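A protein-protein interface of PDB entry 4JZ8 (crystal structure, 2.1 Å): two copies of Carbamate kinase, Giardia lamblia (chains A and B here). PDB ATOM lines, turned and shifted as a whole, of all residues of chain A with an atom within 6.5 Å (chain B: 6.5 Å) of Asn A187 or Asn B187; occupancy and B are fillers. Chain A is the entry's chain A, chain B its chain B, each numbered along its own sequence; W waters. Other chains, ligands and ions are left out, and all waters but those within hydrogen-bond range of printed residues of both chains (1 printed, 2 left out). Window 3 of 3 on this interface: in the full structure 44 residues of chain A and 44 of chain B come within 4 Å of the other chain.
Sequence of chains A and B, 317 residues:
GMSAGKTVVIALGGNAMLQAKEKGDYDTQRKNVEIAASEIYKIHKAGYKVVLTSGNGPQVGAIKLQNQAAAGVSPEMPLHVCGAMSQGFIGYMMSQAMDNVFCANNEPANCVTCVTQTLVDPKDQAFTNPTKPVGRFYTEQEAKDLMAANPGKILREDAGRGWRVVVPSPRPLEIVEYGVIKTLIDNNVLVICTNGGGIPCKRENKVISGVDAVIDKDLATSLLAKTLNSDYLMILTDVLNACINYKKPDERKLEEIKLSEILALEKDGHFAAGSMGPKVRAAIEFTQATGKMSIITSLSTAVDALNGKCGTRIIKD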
ATOM      1  N   LYS A  49      19.094  31.031 -26.456  1.00  0.00           N
ATOM      2  CA  LYS A  49      18.991  29.580 -26.564  1.00  0.00           C
ATOM      3  C   LYS A  49      17.740  29.155 -25.769  1.00  0.00           C
ATOM      4  O   LYS A  49      17.398  29.771 -24.725  1.00  0.00           O
ATOM      5  CB  LYS A  49      20.243  28.885 -26.059  1.00  0.00           C
ATOM      6  CG  LYS A  49      21.523  29.311 -26.764  1.00  0.00           C
ATOM      7  CD  LYS A  49      22.514  28.135 -26.869  1.00  0.00           C
ATOM      8  CE  LYS A  49      23.933  28.528 -26.515  1.00  0.00           C
ATOM      9  NZ  LYS A  49      24.697  27.389 -25.920  1.00  0.00           N
ATOM     10  N   ASN A 110      16.144  23.557 -36.656  1.00  0.00           N
ATOM     11  CA  ASN A 110      17.219  23.149 -35.768  1.00  0.00           C
ATOM     12  C   ASN A 110      16.636  22.811 -34.405  1.00  0.00           C
ATOM     13  O   ASN A 110      16.955  23.444 -33.399  1.00  0.00           O
ATOM     14  CB  ASN A 110      18.258  24.261 -35.648  1.00  0.00           C
ATOM     15  CG  ASN A 110      19.527  23.774 -35.027  1.00  0.00           C
ATOM     16  OD1 ASN A 110      19.876  22.589 -35.178  1.00  0.00           O
ATOM     17  ND2 ASN A 110      20.238  24.665 -34.313  1.00  0.00           N
ATOM     18  N   LYS A 182      22.183  19.089 -22.197  1.00  0.00           N
ATOM     19  CA  LYS A 182      23.211  20.157 -22.142  1.00  0.00           C
ATOM     20  C   LYS A 182      24.103  20.159 -23.377  1.00  0.00           C
ATOM     21  O   LYS A 182      24.563  21.212 -23.817  1.00  0.00           O
ATOM     22  CB  LYS A 182      24.074  19.998 -20.894  1.00  0.00           C
ATOM     23  CG  LYS A 182      25.341  20.865 -20.904  1.00  0.00           C
ATOM     24  CD  LYS A 182      25.061  22.314 -20.453  1.00  0.00           C
ATOM     25  CE  LYS A 182      26.416  23.076 -20.274  1.00  0.00           C
ATOM     26  NZ  LYS A 182      27.546  22.071 -20.191  1.00  0.00           N
ATOM     27  N   THR A 183      24.407  18.966 -23.901  1.00  0.00           N
ATOM     28  CA  THR A 183      25.174  18.852 -25.143  1.00  0.00           C
ATOM     29  C   THR A 183      24.451  19.469 -26.340  1.00  0.00           C
ATOM     30  O   THR A 183      25.054  20.157 -27.162  1.00  0.00           O
ATOM     31  CB  THR A 183      25.503  17.387 -25.462  1.00  0.00           C
ATOM     32  OG1 THR A 183      26.364  16.878 -24.438  1.00  0.00           O
ATOM     33  CG2 THR A 183      26.225  17.265 -26.821  1.00  0.00           C
ATOM     34  N   LEU A 184      23.154  19.236 -26.448  1.00  0.00           N
ATOM     35  CA  LEU A 184      22.371  19.832 -27.535  1.00  0.00           C
ATOM     36  C   LEU A 184      22.350  21.368 -27.443  1.00  0.00           C
ATOM     37  O   LEU A 184      22.582  22.086 -28.436  1.00  0.00           O
ATOM     38  CB  LEU A 184      20.937  19.276 -27.503  1.00  0.00           C
ATOM     39  CG  LEU A 184      20.851  17.817 -27.994  1.00  0.00           C
ATOM     40  CD1 LEU A 184      19.468  17.141 -27.639  1.00  0.00           C
ATOM     41  CD2 LEU A 184      21.083  17.797 -29.506  1.00  0.00           C
ATOM     42  N   ILE A 185      22.037  21.853 -26.246  1.00  0.00           N
ATOM     43  CA  ILE A 185      22.049  23.267 -25.940  1.00  0.00           C
ATOM     44  C   ILE A 185      23.398  23.925 -26.206  1.00  0.00           C
ATOM     45  O   ILE A 185      23.441  25.023 -26.757  1.00  0.00           O
ATOM     46  CB  ILE A 185      21.771  23.484 -24.494  1.00  0.00           C
ATOM     47  CG1 ILE A 185      20.423  22.918 -24.132  1.00  0.00           C
ATOM     48  CG2 ILE A 185      21.767  24.976 -24.188  1.00  0.00           C
ATOM     49  CD1 ILE A 185      20.188  23.041 -22.619  1.00  0.00           C
ATOM     50  N   ASP A 186      24.481  23.274 -25.780  1.00  0.00           N
ATOM     51  CA  ASP A 186      25.841  23.745 -26.107  1.00  0.00           C
ATOM     52  C   ASP A 186      26.024  23.858 -27.617  1.00  0.00           C
ATOM     53  O   ASP A 186      26.780  24.701 -28.096  1.00  0.00           O
ATOM     54  CB  ASP A 186      26.916  22.816 -25.542  1.00  0.00           C
ATOM     55  CG  ASP A 186      27.041  22.919 -24.038  1.00  0.00           C
ATOM     56  OD1 ASP A 186      26.438  23.862 -23.467  1.00  0.00           O
ATOM     57  OD2 ASP A 186      27.749  22.061 -23.443  1.00  0.00           O
ATOM     58  N   ASN A 187      25.320  23.024 -28.377  1.00  0.00           N
ATOM     59  CA  ASN A 187      25.441  23.109 -29.828  1.00  0.00           C
ATOM     60  C   ASN A 187      24.361  23.913 -30.471  1.00  0.00           C
ATOM     61  O   ASN A 187      24.234  23.898 -31.694  1.00  0.00           O
ATOM     62  CB  ASN A 187      25.538  21.736 -30.482  1.00  0.00           C
ATOM     63  CG  ASN A 187      26.948  21.204 -30.466  1.00  0.00           C
ATOM     64  OD1 ASN A 187      27.407  20.686 -29.447  1.00  0.00           O
ATOM     65  ND2 ASN A 187      27.660  21.366 -31.575  1.00  0.00           N
ATOM     66  N   ASN A 188      23.573  24.603 -29.649  1.00  0.00           N
ATOM     67  CA  ASN A 188      22.602  25.549 -30.165  1.00  0.00           C
ATOM     68  C   ASN A 188      21.343  24.928 -30.786  1.00  0.00           C
ATOM     69  O   ASN A 188      20.667  25.540 -31.611  1.00  0.00           O
ATOM     70  CB  ASN A 188      23.300  26.468 -31.175  1.00  0.00           C
ATOM     71  CG  ASN A 188      24.596  27.063 -30.611  1.00  0.00           C
ATOM     72  OD1 ASN A 188      24.605  27.608 -29.514  1.00  0.00           O
ATOM     73  ND2 ASN A 188      25.692  26.933 -31.350  1.00  0.00           N
ATOM     74  N   VAL A 189      21.021  23.706 -30.399  1.00  0.00           N
ATOM     75  CA  VAL A 189      19.770  23.100 -30.867  1.00  0.00           C
ATOM     76  C   VAL A 189      18.643  23.600 -29.976  1.00  0.00           C
ATOM     77  O   VAL A 189      18.824  23.659 -28.760  1.00  0.00           O
ATOM     78  CB  VAL A 189      19.883  21.556 -30.778  1.00  0.00           C
ATOM     79  CG1 VAL A 189      18.565  20.896 -31.180  1.00  0.00           C
ATOM     80  CG2 VAL A 189      21.027  21.091 -31.644  1.00  0.00           C
ATOM     81  N   SER B   3      35.411   9.587 -29.889  1.00  0.00           N
ATOM     82  CA  SER B   3      35.528  10.430 -31.068  1.00  0.00           C
ATOM     83  C   SER B   3      36.202   9.703 -32.203  1.00  0.00           C
ATOM     84  O   SER B   3      36.073  10.113 -33.360  1.00  0.00           O
ATOM     85  CB  SER B   3      36.331  11.695 -30.745  1.00  0.00           C
ATOM     86  OG  SER B   3      35.664  12.485 -29.779  1.00  0.00           O
ATOM     87  N   LYS B  49      30.720   4.323 -32.900  1.00  0.00           N
ATOM     88  CA  LYS B  49      29.556   5.204 -32.652  1.00  0.00           C
ATOM     89  C   LYS B  49      28.313   4.533 -33.224  1.00  0.00           C
ATOM     90  O   LYS B  49      28.352   3.995 -34.328  1.00  0.00           O
ATOM     91  CB  LYS B  49      29.699   6.583 -33.306  1.00  0.00           C
ATOM     92  CG  LYS B  49      30.814   7.499 -32.744  1.00  0.00           C
ATOM     93  CD  LYS B  49      30.844   8.876 -33.467  1.00  0.00           C
ATOM     94  CE  LYS B  49      32.287   9.417 -33.588  1.00  0.00           C
ATOM     95  NZ  LYS B  49      32.386  10.886 -33.945  1.00  0.00           N
ATOM     96  N   ASN B 110      24.889   7.764 -21.654  1.00  0.00           N
ATOM     97  CA  ASN B 110      25.092   8.749 -22.707  1.00  0.00           C
ATOM     98  C   ASN B 110      24.294   8.316 -23.928  1.00  0.00           C
ATOM     99  O   ASN B 110      24.850   8.072 -24.986  1.00  0.00           O
ATOM    100  CB  ASN B 110      26.591   8.858 -23.040  1.00  0.00           C
ATOM    101  CG  ASN B 110      26.933  10.095 -23.897  1.00  0.00           C
ATOM    102  OD1 ASN B 110      26.230  11.129 -23.871  1.00  0.00           O
ATOM    103  ND2 ASN B 110      28.009   9.987 -24.662  1.00  0.00           N
ATOM    104  N   LYS B 182      23.121  14.082 -36.545  1.00  0.00           N
ATOM    105  CA  LYS B 182      24.560  14.283 -36.801  1.00  0.00           C
ATOM    106  C   LYS B 182      25.268  15.021 -35.660  1.00  0.00           C
ATOM    107  O   LYS B 182      26.324  14.595 -35.215  1.00  0.00           O
ATOM    108  CB  LYS B 182      24.762  15.032 -38.121  1.00  0.00           C
ATOM    109  CG  LYS B 182      26.206  15.212 -38.553  1.00  0.00           C
ATOM    110  CD  LYS B 182      26.521  16.671 -38.920  1.00  0.00           C
ATOM    111  CE  LYS B 182      25.277  17.427 -39.414  1.00  0.00           C
ATOM    112  NZ  LYS B 182      25.343  17.745 -40.876  1.00  0.00           N
ATOM    113  N   THR B 183      24.715  16.142 -35.209  1.00  0.00           N
ATOM    114  CA  THR B 183      25.283  16.852 -34.067  1.00  0.00           C
ATOM    115  C   THR B 183      25.547  15.886 -32.900  1.00  0.00           C
ATOM    116  O   THR B 183      26.611  15.896 -32.276  1.00  0.00           O
ATOM    117  CB  THR B 183      24.310  17.948 -33.596  1.00  0.00           C
ATOM    118  OG1 THR B 183      24.290  19.027 -34.545  1.00  0.00           O
ATOM    119  CG2 THR B 183      24.693  18.490 -32.231  1.00  0.00           C
ATOM    120  N   LEU B 184      24.581  15.017 -32.612  1.00  0.00           N
ATOM    121  CA  LEU B 184      24.689  14.132 -31.449  1.00  0.00           C
ATOM    122  C   LEU B 184      25.779  13.078 -31.644  1.00  0.00           C
ATOM    123  O   LEU B 184      26.623  12.806 -30.753  1.00  0.00           O
ATOM    124  CB  LEU B 184      23.323  13.460 -31.190  1.00  0.00           C
ATOM    125  CG  LEU B 184      22.193  14.306 -30.607  1.00  0.00           C
ATOM    126  CD1 LEU B 184      20.821  13.570 -30.702  1.00  0.00           C
ATOM    127  CD2 LEU B 184      22.479  14.695 -29.149  1.00  0.00           C
ATOM    128  N   ILE B 185      25.761  12.444 -32.806  1.00  0.00           N
ATOM    129  CA  ILE B 185      26.765  11.443 -33.063  1.00  0.00           C
ATOM    130  C   ILE B 185      28.135  12.115 -33.128  1.00  0.00           C
ATOM    131  O   ILE B 185      29.135  11.538 -32.677  1.00  0.00           O
ATOM    132  CB  ILE B 185      26.484  10.646 -34.352  1.00  0.00           C
ATOM    133  CG1 ILE B 185      26.081  11.570 -35.496  1.00  0.00           C
ATOM    134  CG2 ILE B 185      25.370   9.611 -34.128  1.00  0.00           C
ATOM    135  CD1 ILE B 185      25.666  10.792 -36.769  1.00  0.00           C
ATOM    136  N   ASP B 186      28.212  13.321 -33.681  1.00  0.00           N
ATOM    137  CA  ASP B 186      29.534  13.968 -33.703  1.00  0.00           C
ATOM    138  C   ASP B 186      29.960  14.124 -32.255  1.00  0.00           C
ATOM    139  O   ASP B 186      31.165  14.188 -31.954  1.00  0.00           O
ATOM    140  CB  ASP B 186      29.492  15.343 -34.383  1.00  0.00           C
ATOM    141  CG  ASP B 186      29.314  15.253 -35.890  1.00  0.00           C
ATOM    142  OD1 ASP B 186      29.712  14.219 -36.489  1.00  0.00           O
ATOM    143  OD2 ASP B 186      28.760  16.217 -36.469  1.00  0.00           O
ATOM    144  N   ASN B 187      28.965  14.174 -31.358  1.00  0.00           N
ATOM    145  CA  ASN B 187      29.241  14.475 -29.950  1.00  0.00           C
ATOM    146  C   ASN B 187      29.301  13.259 -29.086  1.00  0.00           C
ATOM    147  O   ASN B 187      29.317  13.331 -27.852  1.00  0.00           O
ATOM    148  CB  ASN B 187      28.313  15.562 -29.387  1.00  0.00           C
ATOM    149  CG  ASN B 187      28.868  16.952 -29.645  1.00  0.00           C
ATOM    150  OD1 ASN B 187      29.667  17.484 -28.849  1.00  0.00           O
ATOM    151  ND2 ASN B 187      28.501  17.524 -30.789  1.00  0.00           N
ATOM    152  N   ASN B 188      29.355  12.129 -29.773  1.00  0.00           N
ATOM    153  CA  ASN B 188      29.575  10.842 -29.147  1.00  0.00           C
ATOM    154  C   ASN B 188      28.359  10.362 -28.330  1.00  0.00           C
ATOM    155  O   ASN B 188      28.481   9.520 -27.440  1.00  0.00           O
ATOM    156  CB  ASN B 188      30.869  10.904 -28.329  1.00  0.00           C
ATOM    157  CG  ASN B 188      32.069  11.456 -29.158  1.00  0.00           C
ATOM    158  OD1 ASN B 188      32.090  11.370 -30.391  1.00  0.00           O
ATOM    159  ND2 ASN B 188      33.055  12.024 -28.470  1.00  0.00           N
ATOM    160  N   VAL B 189      27.182  10.892 -28.631  1.00  0.00           N
ATOM    161  CA  VAL B 189      25.979  10.351 -27.987  1.00  0.00           C
ATOM    162  C   VAL B 189      25.509   9.110 -28.758  1.00  0.00           C
ATOM    163  O   VAL B 189      25.509   9.073 -30.002  1.00  0.00           O
ATOM    164  CB  VAL B 189      24.844  11.402 -27.877  1.00  0.00           C
ATOM    165  CG1 VAL B 189      23.526  10.781 -27.276  1.00  0.00           C
ATOM    166  CG2 VAL B 189      25.293  12.617 -27.049  1.00  0.00           C
HETATM  167  O   HOH W   1      29.776  19.892 -28.011  1.00  0.00           O
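Thr A183 touches Asn B187, and with the chains exchanged Asn A187 touches Thr B183. Leu A184 touches its own counterpart, Leu B184. Asn B187 touches its own counterpart, Asn A187. Positions printed for both chains: 49, 110, 182, 183, 184, 185, 186, 187, 188 and 189.
O of Thr A183 sits close to OD1 of Asn A187 (3.3 Å). N of Val B189 lies within hydrogen-bond range of O of Leu B184 (2.9 Å). The backbone carbonyl oxygen of Leu A184 sits at hydrogen-bond distance from the backbone NH of Val A189, at 3.0 Å. The side-chain amide nitrogen (ND2) of Asn B187 is in hydrogen-bond range of the backbone carbonyl oxygen (O) of Thr B183 (2.9 Å).
Water W1 bridges the side-chain amide oxygen (OD1) of Asn B187 and the side-chain amide oxygen (OD1) of Asn A187.
Printed residues of chain B within 4 Å of Thr A183: Asn B187 (3.7 Å). Printed residues of chain B within 4 Å of Leu A184: Leu B184 (3.4 Å). Asn A187 touches just these residues of chain B: Thr B183 (3.8 Å) and Asn B187 (3.6 Å). Asn B110 touches none of the printed residues of chain A. Of the printed residues of chain A, Thr B183 touches Asn A187. Of the printed residues of chain A, Leu B184 touches Leu A184. Asn B187 touches just these residues of chain A: Thr A183 and Asn A187. Asn B188 touches none of the printed residues of chain A. The nearest printed residue of chain B that does not touch Asn A187 is Asp B186 (6.9 Å). The nearest printed residue of chain B that does not touch Leu A184 is Thr B183 (4.6 Å).
Among the printed residues, pairs that only touch across the chains: Leu A184 with Leu B184 (3.4 Å), Asn A187 with Asn B187 (3.6 Å), Thr A183 with Asn B187 (3.7 Å) and Asn A187 with Thr B183 (3.8 Å).
Of the 11 printed residues of chain B, 3 touch a printed residue of chain A. Of the 10 printed residues of chain A, 3 touch a printed residue of chain B. Hydrophobic or aromatic side chains of chain A that line the printed part of chain B: Leu A184. Along chain A the printed residues that touch a printed residue of chain B span positions 183 to 187. Among the printed residues, no Asp or Glu carboxylate lies within 4 Å of a Lys or Arg side-chain nitrogen of the other chain.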
